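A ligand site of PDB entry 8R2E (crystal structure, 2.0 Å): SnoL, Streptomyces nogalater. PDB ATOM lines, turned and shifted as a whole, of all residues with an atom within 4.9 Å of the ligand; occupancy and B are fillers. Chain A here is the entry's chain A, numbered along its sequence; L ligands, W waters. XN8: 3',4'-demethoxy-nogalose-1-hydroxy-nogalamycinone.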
ATOM      1  N   MET A  22      13.632  11.897  -0.939  1.00  0.00           N
ATOM      2  CA  MET A  22      12.249  12.279  -0.906  1.00  0.00           C
ATOM      3  C   MET A  22      12.037  13.648  -1.557  1.00  0.00           C
ATOM      4  O   MET A  22      11.021  13.852  -2.174  1.00  0.00           O
ATOM      5  CB  MET A  22      11.714  12.313   0.560  1.00  0.00           C
ATOM      6  CG  MET A  22      11.754  10.973   1.319  1.00  0.00           C
ATOM      7  SD  MET A  22      11.344  11.272   3.064  1.00  0.00           S
ATOM      8  CE  MET A  22      12.516  10.242   3.872  1.00  0.00           C
ATOM      9  N   VAL A  23      12.950  14.598  -1.376  1.00  0.00           N
ATOM     10  CA  VAL A  23      12.796  15.898  -2.018  1.00  0.00           C
ATOM     11  C   VAL A  23      12.868  15.690  -3.549  1.00  0.00           C
ATOM     12  O   VAL A  23      12.077  16.253  -4.320  1.00  0.00           O
ATOM     13  CB  VAL A  23      13.843  16.926  -1.531  1.00  0.00           C
ATOM     14  CG1 VAL A  23      13.788  18.209  -2.371  1.00  0.00           C
ATOM     15  CG2 VAL A  23      13.611  17.257  -0.077  1.00  0.00           C
ATOM     16  N   TRP A  26       9.682  14.380  -4.953  1.00  0.00           N
ATOM     17  CA  TRP A  26       8.759  15.519  -5.095  1.00  0.00           C
ATOM     18  C   TRP A  26       9.062  16.379  -6.368  1.00  0.00           C
ATOM     19  O   TRP A  26       8.169  16.885  -7.050  1.00  0.00           O
ATOM     20  CB  TRP A  26       8.811  16.475  -3.866  1.00  0.00           C
ATOM     21  CG  TRP A  26       7.868  16.163  -2.711  1.00  0.00           C
ATOM     22  CD1 TRP A  26       8.207  15.692  -1.521  1.00  0.00           C
ATOM     23  CD2 TRP A  26       6.497  16.431  -2.686  1.00  0.00           C
ATOM     24  NE1 TRP A  26       7.088  15.584  -0.718  1.00  0.00           N
ATOM     25  CE2 TRP A  26       6.020  16.030  -1.434  1.00  0.00           C
ATOM     26  CE3 TRP A  26       5.595  16.953  -3.624  1.00  0.00           C
ATOM     27  CZ2 TRP A  26       4.695  16.135  -1.074  1.00  0.00           C
ATOM     28  CZ3 TRP A  26       4.265  17.040  -3.276  1.00  0.00           C
ATOM     29  CH2 TRP A  26       3.820  16.629  -2.012  1.00  0.00           C
ATOM     30  N   VAL A  34       8.032   9.372  -2.545  1.00  0.00           N
ATOM     31  CA  VAL A  34       8.082   9.851  -1.175  1.00  0.00           C
ATOM     32  C   VAL A  34       7.594   8.751  -0.229  1.00  0.00           C
ATOM     33  O   VAL A  34       8.269   8.370   0.706  1.00  0.00           O
ATOM     34  CB  VAL A  34       7.266  11.138  -0.986  1.00  0.00           C
ATOM     35  CG1 VAL A  34       7.353  11.557   0.449  1.00  0.00           C
ATOM     36  CG2 VAL A  34       7.727  12.282  -1.898  1.00  0.00           C
ATOM     37  N   TRP A  38       8.220   5.464   3.811  1.00  0.00           N
ATOM     38  CA  TRP A  38       7.402   5.345   5.007  1.00  0.00           C
ATOM     39  C   TRP A  38       7.436   3.942   5.558  1.00  0.00           C
ATOM     40  O   TRP A  38       7.319   2.996   4.815  1.00  0.00           O
ATOM     41  CB  TRP A  38       5.945   5.666   4.701  1.00  0.00           C
ATOM     42  CG  TRP A  38       5.782   7.070   4.307  1.00  0.00           C
ATOM     43  CD1 TRP A  38       6.762   8.057   4.290  1.00  0.00           C
ATOM     44  CD2 TRP A  38       4.580   7.682   3.943  1.00  0.00           C
ATOM     45  NE1 TRP A  38       6.208   9.233   3.909  1.00  0.00           N
ATOM     46  CE2 TRP A  38       4.868   9.053   3.708  1.00  0.00           C
ATOM     47  CE3 TRP A  38       3.283   7.224   3.816  1.00  0.00           C
ATOM     48  CZ2 TRP A  38       3.906   9.942   3.309  1.00  0.00           C
ATOM     49  CZ3 TRP A  38       2.330   8.107   3.431  1.00  0.00           C
ATOM     50  CH2 TRP A  38       2.644   9.461   3.124  1.00  0.00           C
ATOM     51  N   HIS A  44       1.607  10.299  10.816  1.00  0.00           N
ATOM     52  CA  HIS A  44       1.671  11.658  10.376  1.00  0.00           C
ATOM     53  C   HIS A  44       0.817  12.509  11.266  1.00  0.00           C
ATOM     54  O   HIS A  44      -0.303  12.156  11.525  1.00  0.00           O
ATOM     55  CB  HIS A  44       1.073  11.748   8.995  1.00  0.00           C
ATOM     56  CG  HIS A  44       1.772  10.899   8.001  1.00  0.00           C
ATOM     57  ND1 HIS A  44       2.887  11.327   7.354  1.00  0.00           N
ATOM     58  CD2 HIS A  44       1.561   9.626   7.585  1.00  0.00           C
ATOM     59  CE1 HIS A  44       3.333  10.386   6.546  1.00  0.00           C
ATOM     60  NE2 HIS A  44       2.526   9.346   6.649  1.00  0.00           N
ATOM     61  N   ASP A  46      -1.128  16.236  12.016  1.00  0.00           N
ATOM     62  CA  ASP A  46      -1.595  17.567  11.555  1.00  0.00           C
ATOM     63  C   ASP A  46      -1.173  18.701  12.471  1.00  0.00           C
ATOM     64  O   ASP A  46      -0.556  18.487  13.534  1.00  0.00           O
ATOM     65  CB  ASP A  46      -3.112  17.591  11.301  1.00  0.00           C
ATOM     66  CG  ASP A  46      -3.952  17.409  12.553  1.00  0.00           C
ATOM     67  OD1 ASP A  46      -3.557  17.790  13.695  1.00  0.00           O
ATOM     68  OD2 ASP A  46      -5.059  16.856  12.328  1.00  0.00           O
ATOM     69  N   ASP A  47      -1.512  19.904  12.039  1.00  0.00           N
ATOM     70  CA  ASP A  47      -1.230  21.137  12.773  1.00  0.00           C
ATOM     71  C   ASP A  47      -1.670  21.152  14.221  1.00  0.00           C
ATOM     72  O   ASP A  47      -1.167  21.958  14.970  1.00  0.00           O
ATOM     73  CB  ASP A  47      -1.809  22.370  12.021  1.00  0.00           C
ATOM     74  CG  ASP A  47      -3.324  22.271  11.776  1.00  0.00           C
ATOM     75  OD1 ASP A  47      -3.771  21.657  10.767  1.00  0.00           O
ATOM     76  OD2 ASP A  47      -4.065  22.853  12.577  1.00  0.00           O
ATOM     77  N   VAL A  52      -3.055  11.826  11.254  1.00  0.00           N
ATOM     78  CA  VAL A  52      -3.750  11.808   9.999  1.00  0.00           C
ATOM     79  C   VAL A  52      -3.402  10.505   9.301  1.00  0.00           C
ATOM     80  O   VAL A  52      -2.235  10.136   9.239  1.00  0.00           O
ATOM     81  CB  VAL A  52      -3.251  12.946   9.107  1.00  0.00           C
ATOM     82  CG1 VAL A  52      -4.042  12.959   7.799  1.00  0.00           C
ATOM     83  CG2 VAL A  52      -3.400  14.233   9.836  1.00  0.00           C
ATOM     84  N   VAL A  57      -3.008  11.492   3.859  1.00  0.00           N
ATOM     85  CA  VAL A  57      -1.785  12.183   3.570  1.00  0.00           C
ATOM     86  C   VAL A  57      -1.490  12.053   2.062  1.00  0.00           C
ATOM     87  O   VAL A  57      -1.264  13.052   1.381  1.00  0.00           O
ATOM     88  CB  VAL A  57      -0.647  11.736   4.445  1.00  0.00           C
ATOM     89  CG1 VAL A  57       0.649  12.412   3.996  1.00  0.00           C
ATOM     90  CG2 VAL A  57      -0.917  12.183   5.866  1.00  0.00           C
ATOM     91  N   ARG A  60      -3.668  14.313   0.039  1.00  0.00           N
ATOM     92  CA  ARG A  60      -3.287  15.721   0.022  1.00  0.00           C
ATOM     93  C   ARG A  60      -2.068  15.885  -0.883  1.00  0.00           C
ATOM     94  O   ARG A  60      -2.023  16.833  -1.648  1.00  0.00           O
ATOM     95  CB  ARG A  60      -2.974  16.220   1.431  1.00  0.00           C
ATOM     96  CG  ARG A  60      -4.223  16.307   2.321  1.00  0.00           C
ATOM     97  CD  ARG A  60      -3.840  16.357   3.784  1.00  0.00           C
ATOM     98  NE  ARG A  60      -5.038  16.395   4.625  1.00  0.00           N
ATOM     99  CZ  ARG A  60      -5.069  16.683   5.928  1.00  0.00           C
ATOM    100  NH1 ARG A  60      -3.976  16.988   6.611  1.00  0.00           N
ATOM    101  NH2 ARG A  60      -6.252  16.678   6.557  1.00  0.00           N
ATOM    102  N   MET A  61      -1.132  14.955  -0.835  1.00  0.00           N
ATOM    103  CA  MET A  61       0.094  15.043  -1.650  1.00  0.00           C
ATOM    104  C   MET A  61      -0.219  14.963  -3.116  1.00  0.00           C
ATOM    105  O   MET A  61       0.362  15.692  -3.922  1.00  0.00           O
ATOM    106  CB  MET A  61       1.107  13.951  -1.311  1.00  0.00           C
ATOM    107  CG  MET A  61       1.770  14.150   0.068  1.00  0.00           C
ATOM    108  SD  MET A  61       2.617  12.690   0.720  1.00  0.00           S
ATOM    109  CE  MET A  61       4.201  12.961   0.053  1.00  0.00           C
ATOM    110  N   ALA A  64      -1.614  18.177  -4.332  1.00  0.00           N
ATOM    111  CA  ALA A  64      -0.619  19.261  -4.493  1.00  0.00           C
ATOM    112  C   ALA A  64       0.073  19.102  -5.846  1.00  0.00           C
ATOM    113  O   ALA A  64       0.274  20.090  -6.561  1.00  0.00           O
ATOM    114  CB  ALA A  64       0.389  19.235  -3.362  1.00  0.00           C
ATOM    115  N   LEU A  71       5.800  22.451  -9.519  1.00  0.00           N
ATOM    116  CA  LEU A  71       6.428  22.740  -8.265  1.00  0.00           C
ATOM    117  C   LEU A  71       7.920  22.340  -8.204  1.00  0.00           C
ATOM    118  O   LEU A  71       8.381  21.360  -8.804  1.00  0.00           O
ATOM    119  CB  LEU A  71       5.598  22.204  -7.081  1.00  0.00           C
ATOM    120  CG  LEU A  71       5.662  20.701  -6.895  1.00  0.00           C
ATOM    121  CD1 LEU A  71       6.880  20.249  -6.053  1.00  0.00           C
ATOM    122  CD2 LEU A  71       4.378  20.191  -6.252  1.00  0.00           C
ATOM    123  N   LEU A  73      11.102  22.260  -5.147  1.00  0.00           N
ATOM    124  CA  LEU A  73      11.430  22.411  -3.723  1.00  0.00           C
ATOM    125  C   LEU A  73      12.896  22.657  -3.591  1.00  0.00           C
ATOM    126  O   LEU A  73      13.688  21.902  -4.150  1.00  0.00           O
ATOM    127  CB  LEU A  73      11.068  21.139  -2.943  1.00  0.00           C
ATOM    128  CG  LEU A  73       9.650  20.632  -3.066  1.00  0.00           C
ATOM    129  CD1 LEU A  73       9.482  19.483  -2.087  1.00  0.00           C
ATOM    130  CD2 LEU A  73       8.737  21.784  -2.727  1.00  0.00           C
ATOM    131  N   ILE A  89      12.329  24.133   3.813  1.00  0.00           N
ATOM    132  CA  ILE A  89      12.201  23.969   2.384  1.00  0.00           C
ATOM    133  C   ILE A  89      11.365  25.120   1.859  1.00  0.00           C
ATOM    134  O   ILE A  89      10.422  25.532   2.508  1.00  0.00           O
ATOM    135  CB  ILE A  89      11.514  22.664   2.029  1.00  0.00           C
ATOM    136  CG1 ILE A  89      12.335  21.485   2.528  1.00  0.00           C
ATOM    137  CG2 ILE A  89      11.280  22.550   0.539  1.00  0.00           C
ATOM    138  CD1 ILE A  89      11.610  20.147   2.625  1.00  0.00           C
ATOM    139  N   CYS A  91       9.062  26.001  -1.473  1.00  0.00           N
ATOM    140  CA  CYS A  91       8.385  25.497  -2.659  1.00  0.00           C
ATOM    141  C   CYS A  91       7.923  26.690  -3.494  1.00  0.00           C
ATOM    142  O   CYS A  91       7.387  27.625  -2.965  1.00  0.00           O
ATOM    143  CB  CYS A  91       7.159  24.637  -2.287  1.00  0.00           C
ATOM    144  SG  CYS A  91       6.133  24.055  -3.687  1.00  0.00           S
ATOM    145  N   PHE A  99      -6.872  23.465  -4.930  1.00  0.00           N
ATOM    146  CA  PHE A  99      -6.146  22.840  -3.832  1.00  0.00           C
ATOM    147  C   PHE A  99      -6.811  23.180  -2.514  1.00  0.00           C
ATOM    148  O   PHE A  99      -6.912  24.343  -2.191  1.00  0.00           O
ATOM    149  CB  PHE A  99      -4.694  23.296  -3.821  1.00  0.00           C
ATOM    150  CG  PHE A  99      -3.873  22.667  -2.721  1.00  0.00           C
ATOM    151  CD1 PHE A  99      -3.489  21.349  -2.795  1.00  0.00           C
ATOM    152  CD2 PHE A  99      -3.461  23.429  -1.621  1.00  0.00           C
ATOM    153  CE1 PHE A  99      -2.744  20.757  -1.757  1.00  0.00           C
ATOM    154  CE2 PHE A  99      -2.705  22.876  -0.593  1.00  0.00           C
ATOM    155  CZ  PHE A  99      -2.351  21.529  -0.664  1.00  0.00           C
ATOM    156  N   MET A 100      -7.223  22.167  -1.770  1.00  0.00           N
ATOM    157  CA  MET A 100      -7.833  22.392  -0.433  1.00  0.00           C
ATOM    158  C   MET A 100      -8.887  23.444  -0.561  1.00  0.00           C
ATOM    159  O   MET A 100      -8.894  24.450   0.143  1.00  0.00           O
ATOM    160  CB  MET A 100      -6.749  22.762   0.580  1.00  0.00           C
ATOM    161  CG  MET A 100      -5.677  21.684   0.651  1.00  0.00           C
ATOM    162  SD  MET A 100      -6.369  20.145   1.314  1.00  0.00           S
ATOM    163  CE  MET A 100      -5.689  18.872   0.274  1.00  0.00           C
ATOM    164  N   TRP A 111       6.105  29.283  -0.919  1.00  0.00           N
ATOM    165  CA  TRP A 111       5.969  29.189   0.517  1.00  0.00           C
ATOM    166  C   TRP A 111       7.159  28.413   1.078  1.00  0.00           C
ATOM    167  O   TRP A 111       7.827  27.662   0.343  1.00  0.00           O
ATOM    168  CB  TRP A 111       4.623  28.561   0.938  1.00  0.00           C
ATOM    169  CG  TRP A 111       4.393  27.199   0.472  1.00  0.00           C
ATOM    170  CD1 TRP A 111       4.849  26.097   1.032  1.00  0.00           C
ATOM    171  CD2 TRP A 111       3.693  26.812  -0.699  1.00  0.00           C
ATOM    172  NE1 TRP A 111       4.479  24.973   0.296  1.00  0.00           N
ATOM    173  CE2 TRP A 111       3.740  25.403  -0.767  1.00  0.00           C
ATOM    174  CE3 TRP A 111       3.004  27.515  -1.692  1.00  0.00           C
ATOM    175  CZ2 TRP A 111       3.141  24.669  -1.793  1.00  0.00           C
ATOM    176  CZ3 TRP A 111       2.382  26.786  -2.702  1.00  0.00           C
ATOM    177  CH2 TRP A 111       2.466  25.372  -2.751  1.00  0.00           C
ATOM    178  N   TYR A 113       8.545  26.047   4.516  1.00  0.00           N
ATOM    179  CA  TYR A 113       8.041  25.170   5.568  1.00  0.00           C
ATOM    180  C   TYR A 113       9.082  24.305   6.223  1.00  0.00           C
ATOM    181  O   TYR A 113      10.163  24.156   5.703  1.00  0.00           O
ATOM    182  CB  TYR A 113       6.939  24.284   5.025  1.00  0.00           C
ATOM    183  CG  TYR A 113       7.264  23.306   3.929  1.00  0.00           C
ATOM    184  CD1 TYR A 113       7.461  21.961   4.196  1.00  0.00           C
ATOM    185  CD2 TYR A 113       7.321  23.757   2.587  1.00  0.00           C
ATOM    186  CE1 TYR A 113       7.705  21.073   3.156  1.00  0.00           C
ATOM    187  CE2 TYR A 113       7.563  22.894   1.560  1.00  0.00           C
ATOM    188  CZ  TYR A 113       7.763  21.567   1.839  1.00  0.00           C
ATOM    189  OH  TYR A 113       8.003  20.744   0.795  1.00  0.00           O
ATOM    190  N   GLU A 115       9.865  20.367   7.529  1.00  0.00           N
ATOM    191  CA  GLU A 115       9.534  18.967   7.591  1.00  0.00           C
ATOM    192  C   GLU A 115      10.371  18.367   8.666  1.00  0.00           C
ATOM    193  O   GLU A 115      11.598  18.518   8.614  1.00  0.00           O
ATOM    194  CB  GLU A 115       9.917  18.296   6.278  1.00  0.00           C
ATOM    195  CG  GLU A 115       8.969  18.576   5.147  1.00  0.00           C
ATOM    196  CD  GLU A 115       7.587  17.967   5.376  1.00  0.00           C
ATOM    197  OE1 GLU A 115       7.543  16.866   5.989  1.00  0.00           O
ATOM    198  OE2 GLU A 115       6.571  18.579   4.993  1.00  0.00           O
ATOM    199  N   LEU A 117      11.237  14.583  10.304  1.00  0.00           N
ATOM    200  CA  LEU A 117      11.111  13.142  10.115  1.00  0.00           C
ATOM    201  C   LEU A 117      11.877  12.347  11.166  1.00  0.00           C
ATOM    202  O   LEU A 117      13.009  12.618  11.437  1.00  0.00           O
ATOM    203  CB  LEU A 117      11.564  12.736   8.736  1.00  0.00           C
ATOM    204  CG  LEU A 117      10.732  13.424   7.676  1.00  0.00           C
ATOM    205  CD1 LEU A 117      11.514  13.774   6.486  1.00  0.00           C
ATOM    206  CD2 LEU A 117       9.525  12.646   7.288  1.00  0.00           C
ATOM    207  N   HIS A 128       6.121  11.740  11.516  1.00  0.00           N
ATOM    208  CA  HIS A 128       6.278  12.824  10.571  1.00  0.00           C
ATOM    209  C   HIS A 128       5.484  14.051  11.011  1.00  0.00           C
ATOM    210  O   HIS A 128       4.307  13.952  11.292  1.00  0.00           O
ATOM    211  CB  HIS A 128       5.845  12.348   9.183  1.00  0.00           C
ATOM    212  CG  HIS A 128       5.673  13.458   8.200  1.00  0.00           C
ATOM    213  ND1 HIS A 128       4.524  13.629   7.458  1.00  0.00           N
ATOM    214  CD2 HIS A 128       6.464  14.510   7.913  1.00  0.00           C
ATOM    215  CE1 HIS A 128       4.637  14.713   6.707  1.00  0.00           C
ATOM    216  NE2 HIS A 128       5.811  15.263   6.957  1.00  0.00           N
ATOM    217  N   ASP A 130       5.015  18.525  10.188  1.00  0.00           N
ATOM    218  CA  ASP A 130       5.244  19.694   9.296  1.00  0.00           C
ATOM    219  C   ASP A 130       4.861  20.990  10.047  1.00  0.00           C
ATOM    220  O   ASP A 130       4.052  20.989  10.979  1.00  0.00           O
ATOM    221  CB  ASP A 130       4.396  19.749   8.018  1.00  0.00           C
ATOM    222  CG  ASP A 130       4.002  18.393   7.406  1.00  0.00           C
ATOM    223  OD1 ASP A 130       4.700  17.852   6.498  1.00  0.00           O
ATOM    224  OD2 ASP A 130       2.908  17.913   7.751  1.00  0.00           O
ATOM    225  N   PHE A 132       3.765  24.562   8.254  1.00  0.00           N
ATOM    226  CA  PHE A 132       3.575  25.346   7.046  1.00  0.00           C
ATOM    227  C   PHE A 132       3.065  26.751   7.342  1.00  0.00           C
ATOM    228  O   PHE A 132       2.154  26.958   8.153  1.00  0.00           O
ATOM    229  CB  PHE A 132       2.558  24.637   6.137  1.00  0.00           C
ATOM    230  CG  PHE A 132       3.152  23.505   5.334  1.00  0.00           C
ATOM    231  CD1 PHE A 132       3.192  22.233   5.846  1.00  0.00           C
ATOM    232  CD2 PHE A 132       3.651  23.731   4.086  1.00  0.00           C
ATOM    233  CE1 PHE A 132       3.695  21.180   5.100  1.00  0.00           C
ATOM    234  CE2 PHE A 132       4.164  22.688   3.338  1.00  0.00           C
ATOM    235  CZ  PHE A 132       4.184  21.397   3.853  1.00  0.00           C
ATOM    236  N   PHE A 134       1.195  28.793   4.988  1.00  0.00           N
ATOM    237  CA  PHE A 134       0.471  28.788   3.749  1.00  0.00           C
ATOM    238  C   PHE A 134      -0.175  30.140   3.454  1.00  0.00           C
ATOM    239  O   PHE A 134      -0.934  30.229   2.494  1.00  0.00           O
ATOM    240  CB  PHE A 134      -0.645  27.739   3.779  1.00  0.00           C
ATOM    241  CG  PHE A 134      -0.208  26.372   3.436  1.00  0.00           C
ATOM    242  CD1 PHE A 134       0.510  26.142   2.277  1.00  0.00           C
ATOM    243  CD2 PHE A 134      -0.557  25.310   4.214  1.00  0.00           C
ATOM    244  CE1 PHE A 134       0.925  24.866   1.921  1.00  0.00           C
ATOM    245  CE2 PHE A 134      -0.166  23.996   3.848  1.00  0.00           C
ATOM    246  CZ  PHE A 134       0.580  23.780   2.701  1.00  0.00           C
HETATM  247  CBP XN8 L   1      -0.569  15.858   6.446  1.00  0.00           C
HETATM  248  OBO XN8 L   1      -1.192  16.893   5.696  1.00  0.00           O
HETATM  249  CAD XN8 L   1      -0.254  17.920   5.365  1.00  0.00           C
HETATM  250  CAC XN8 L   1      -0.724  19.213   5.958  1.00  0.00           C
HETATM  251  CAK XN8 L   1       0.430  20.217   5.964  1.00  0.00           C
HETATM  252  OAJ XN8 L   1      -1.093  18.989   7.297  1.00  0.00           O
HETATM  253  CAB XN8 L   1      -1.924  19.713   5.232  1.00  0.00           C
HETATM  254  OAG XN8 L   1      -2.265  20.978   5.705  1.00  0.00           O
HETATM  255  CAA XN8 L   1      -1.630  19.835   3.777  1.00  0.00           C
HETATM  256  CAL XN8 L   1      -2.899  20.267   3.075  1.00  0.00           C
HETATM  257  OAF XN8 L   1      -1.268  18.548   3.305  1.00  0.00           O
HETATM  258  CAE XN8 L   1      -0.131  17.958   3.863  1.00  0.00           C
HETATM  259  OAH XN8 L   1       1.105  18.577   3.514  1.00  0.00           O
HETATM  260  CBD XN8 L   1       1.492  18.344   2.235  1.00  0.00           C
HETATM  261  CBE XN8 L   1       0.890  19.301   1.375  1.00  0.00           C
HETATM  262  CBF XN8 L   1       1.867  19.899   0.341  1.00  0.00           C
HETATM  263  CBM XN8 L   1       1.252  21.195  -0.293  1.00  0.00           C
HETATM  264  OBL XN8 L   1       1.959  18.863  -0.615  1.00  0.00           O
HETATM  265  CAY XN8 L   1       2.820  17.978   2.141  1.00  0.00           C
HETATM  266  CAX XN8 L   1       3.343  16.801   2.659  1.00  0.00           C
HETATM  267  OBN XN8 L   1       2.493  15.904   3.194  1.00  0.00           O
HETATM  268  CAT XN8 L   1       4.694  16.472   2.625  1.00  0.00           C
HETATM  269  CAS XN8 L   1       5.151  15.258   3.121  1.00  0.00           C
HETATM  270  OBC XN8 L   1       4.334  14.462   3.605  1.00  0.00           O
HETATM  271  CAP XN8 L   1       6.493  14.948   3.093  1.00  0.00           C
HETATM  272  CAO XN8 L   1       6.957  13.741   3.610  1.00  0.00           C
HETATM  273  OAW XN8 L   1       6.037  12.859   4.113  1.00  0.00           O
HETATM  274  CAN XN8 L   1       8.294  13.398   3.599  1.00  0.00           C
HETATM  275  CAM XN8 L   1       9.185  14.280   3.040  1.00  0.00           C
HETATM  276  CAR XN8 L   1       8.730  15.467   2.517  1.00  0.00           C
HETATM  277  OAS XN8 L   1       9.627  16.299   1.997  1.00  0.00           O
HETATM  278  CAQ XN8 L   1       7.378  15.837   2.534  1.00  0.00           C
HETATM  279  CAV XN8 L   1       6.910  17.082   2.037  1.00  0.00           C
HETATM  280  OBB XN8 L   1       7.680  17.902   1.525  1.00  0.00           O
HETATM  281  CAU XN8 L   1       5.564  17.389   2.086  1.00  0.00           C
HETATM  282  CBA XN8 L   1       5.081  18.590   1.528  1.00  0.00           C
HETATM  283  CAZ XN8 L   1       3.721  18.953   1.589  1.00  0.00           C
HETATM  284  CBG XN8 L   1       3.220  20.109   0.929  1.00  0.00           C
HETATM  285  CBH XN8 L   1       4.098  20.793   0.080  1.00  0.00           C
HETATM  286  OBJ XN8 L   1       4.598  21.813  -0.087  1.00  0.00           O
HETATM  287  OBI XN8 L   1       4.234  20.387  -0.916  1.00  0.00           O
HETATM  288  CBK XN8 L   1       5.338  20.311  -1.989  1.00  0.00           C
HETATM  289  O   HOH W   1      -3.366  19.266   8.686  1.00  0.00           O
HETATM  290  O   HOH W   2       0.726  18.012   8.962  1.00  0.00           O
HETATM  291  O   HOH W   3      -5.592  21.933   5.622  1.00  0.00           O
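An oxygen (OBO) of the ligand sits at hydrogen-bond distance from the guanidinium group (NH1) of Arg 60, 2.9 Å away.
OH of Tyr 113 is in hydrogen-bond range of OBB of the ligand (3.0 Å).
The indole nitrogen (NE1) of Trp 26 lies close to an oxygen (OBB) of the ligand, 3.3 Å away.
NE1 of Trp 111 lies within hydrogen-bond range of OBJ of the ligand, 3.2 Å away.
N of Tyr 113 is in hydrogen-bond range of O of Ile 89 (2.8 Å).
A ring nitrogen (NE2) of His 128 is in hydrogen-bond range of the side-chain carboxylate (OE1) of Glu 115, at 2.6 Å.
A ring nitrogen (NE2) of His 128 lies within hydrogen-bond range of the side-chain carboxylate (OD1) of Asp 130 (2.9 Å).
A ring nitrogen (ND1) of His 128 sits at hydrogen-bond distance from a ring nitrogen (ND1) of His 44 (2.8 Å).
O of Trp 111 sits at hydrogen-bond distance from N of Cys 91 (2.8 Å).
The side-chain carboxylate (OE2) of Glu 115 lies close to the side-chain carboxylate (OD1) of Asp 130.
The side-chain sulfur of Met 61 sits close to an oxygen (OBC) of the ligand (3.8 Å).
Residues that only touch the ligand: His 128, Ala 64, Glu 115, Phe 132, Trp 38, Phe 99, Met 22, Val 57, Val 34, Leu 73, Asp 130, Met 100 and Leu 117.
Hydrophobic or aromatic side chains within 4 Å of the ligand: Met 22, Trp 26, Val 34, Trp 38, Val 57, Met 61, Ala 64, Leu 73, Phe 99, Met 100, Trp 111, Tyr 113, Leu 117, His 128 and Phe 132.
Of the 27 residues printed, 18 come within 4 Å of the ligand.
The nearest printed residue that does not touch the ligand is Phe 134 (4.01 Å).
Water W2 lies within hydrogen-bond range of OD2 of Asp 130 (2.5 Å) and OAJ of the ligand (2.7 Å).
Water W1 lies within hydrogen-bond range of OAJ of the ligand (2.7 Å), NH1 of Arg 60 (3.1 Å) and OD1 of Asp 47 (3.2 Å).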
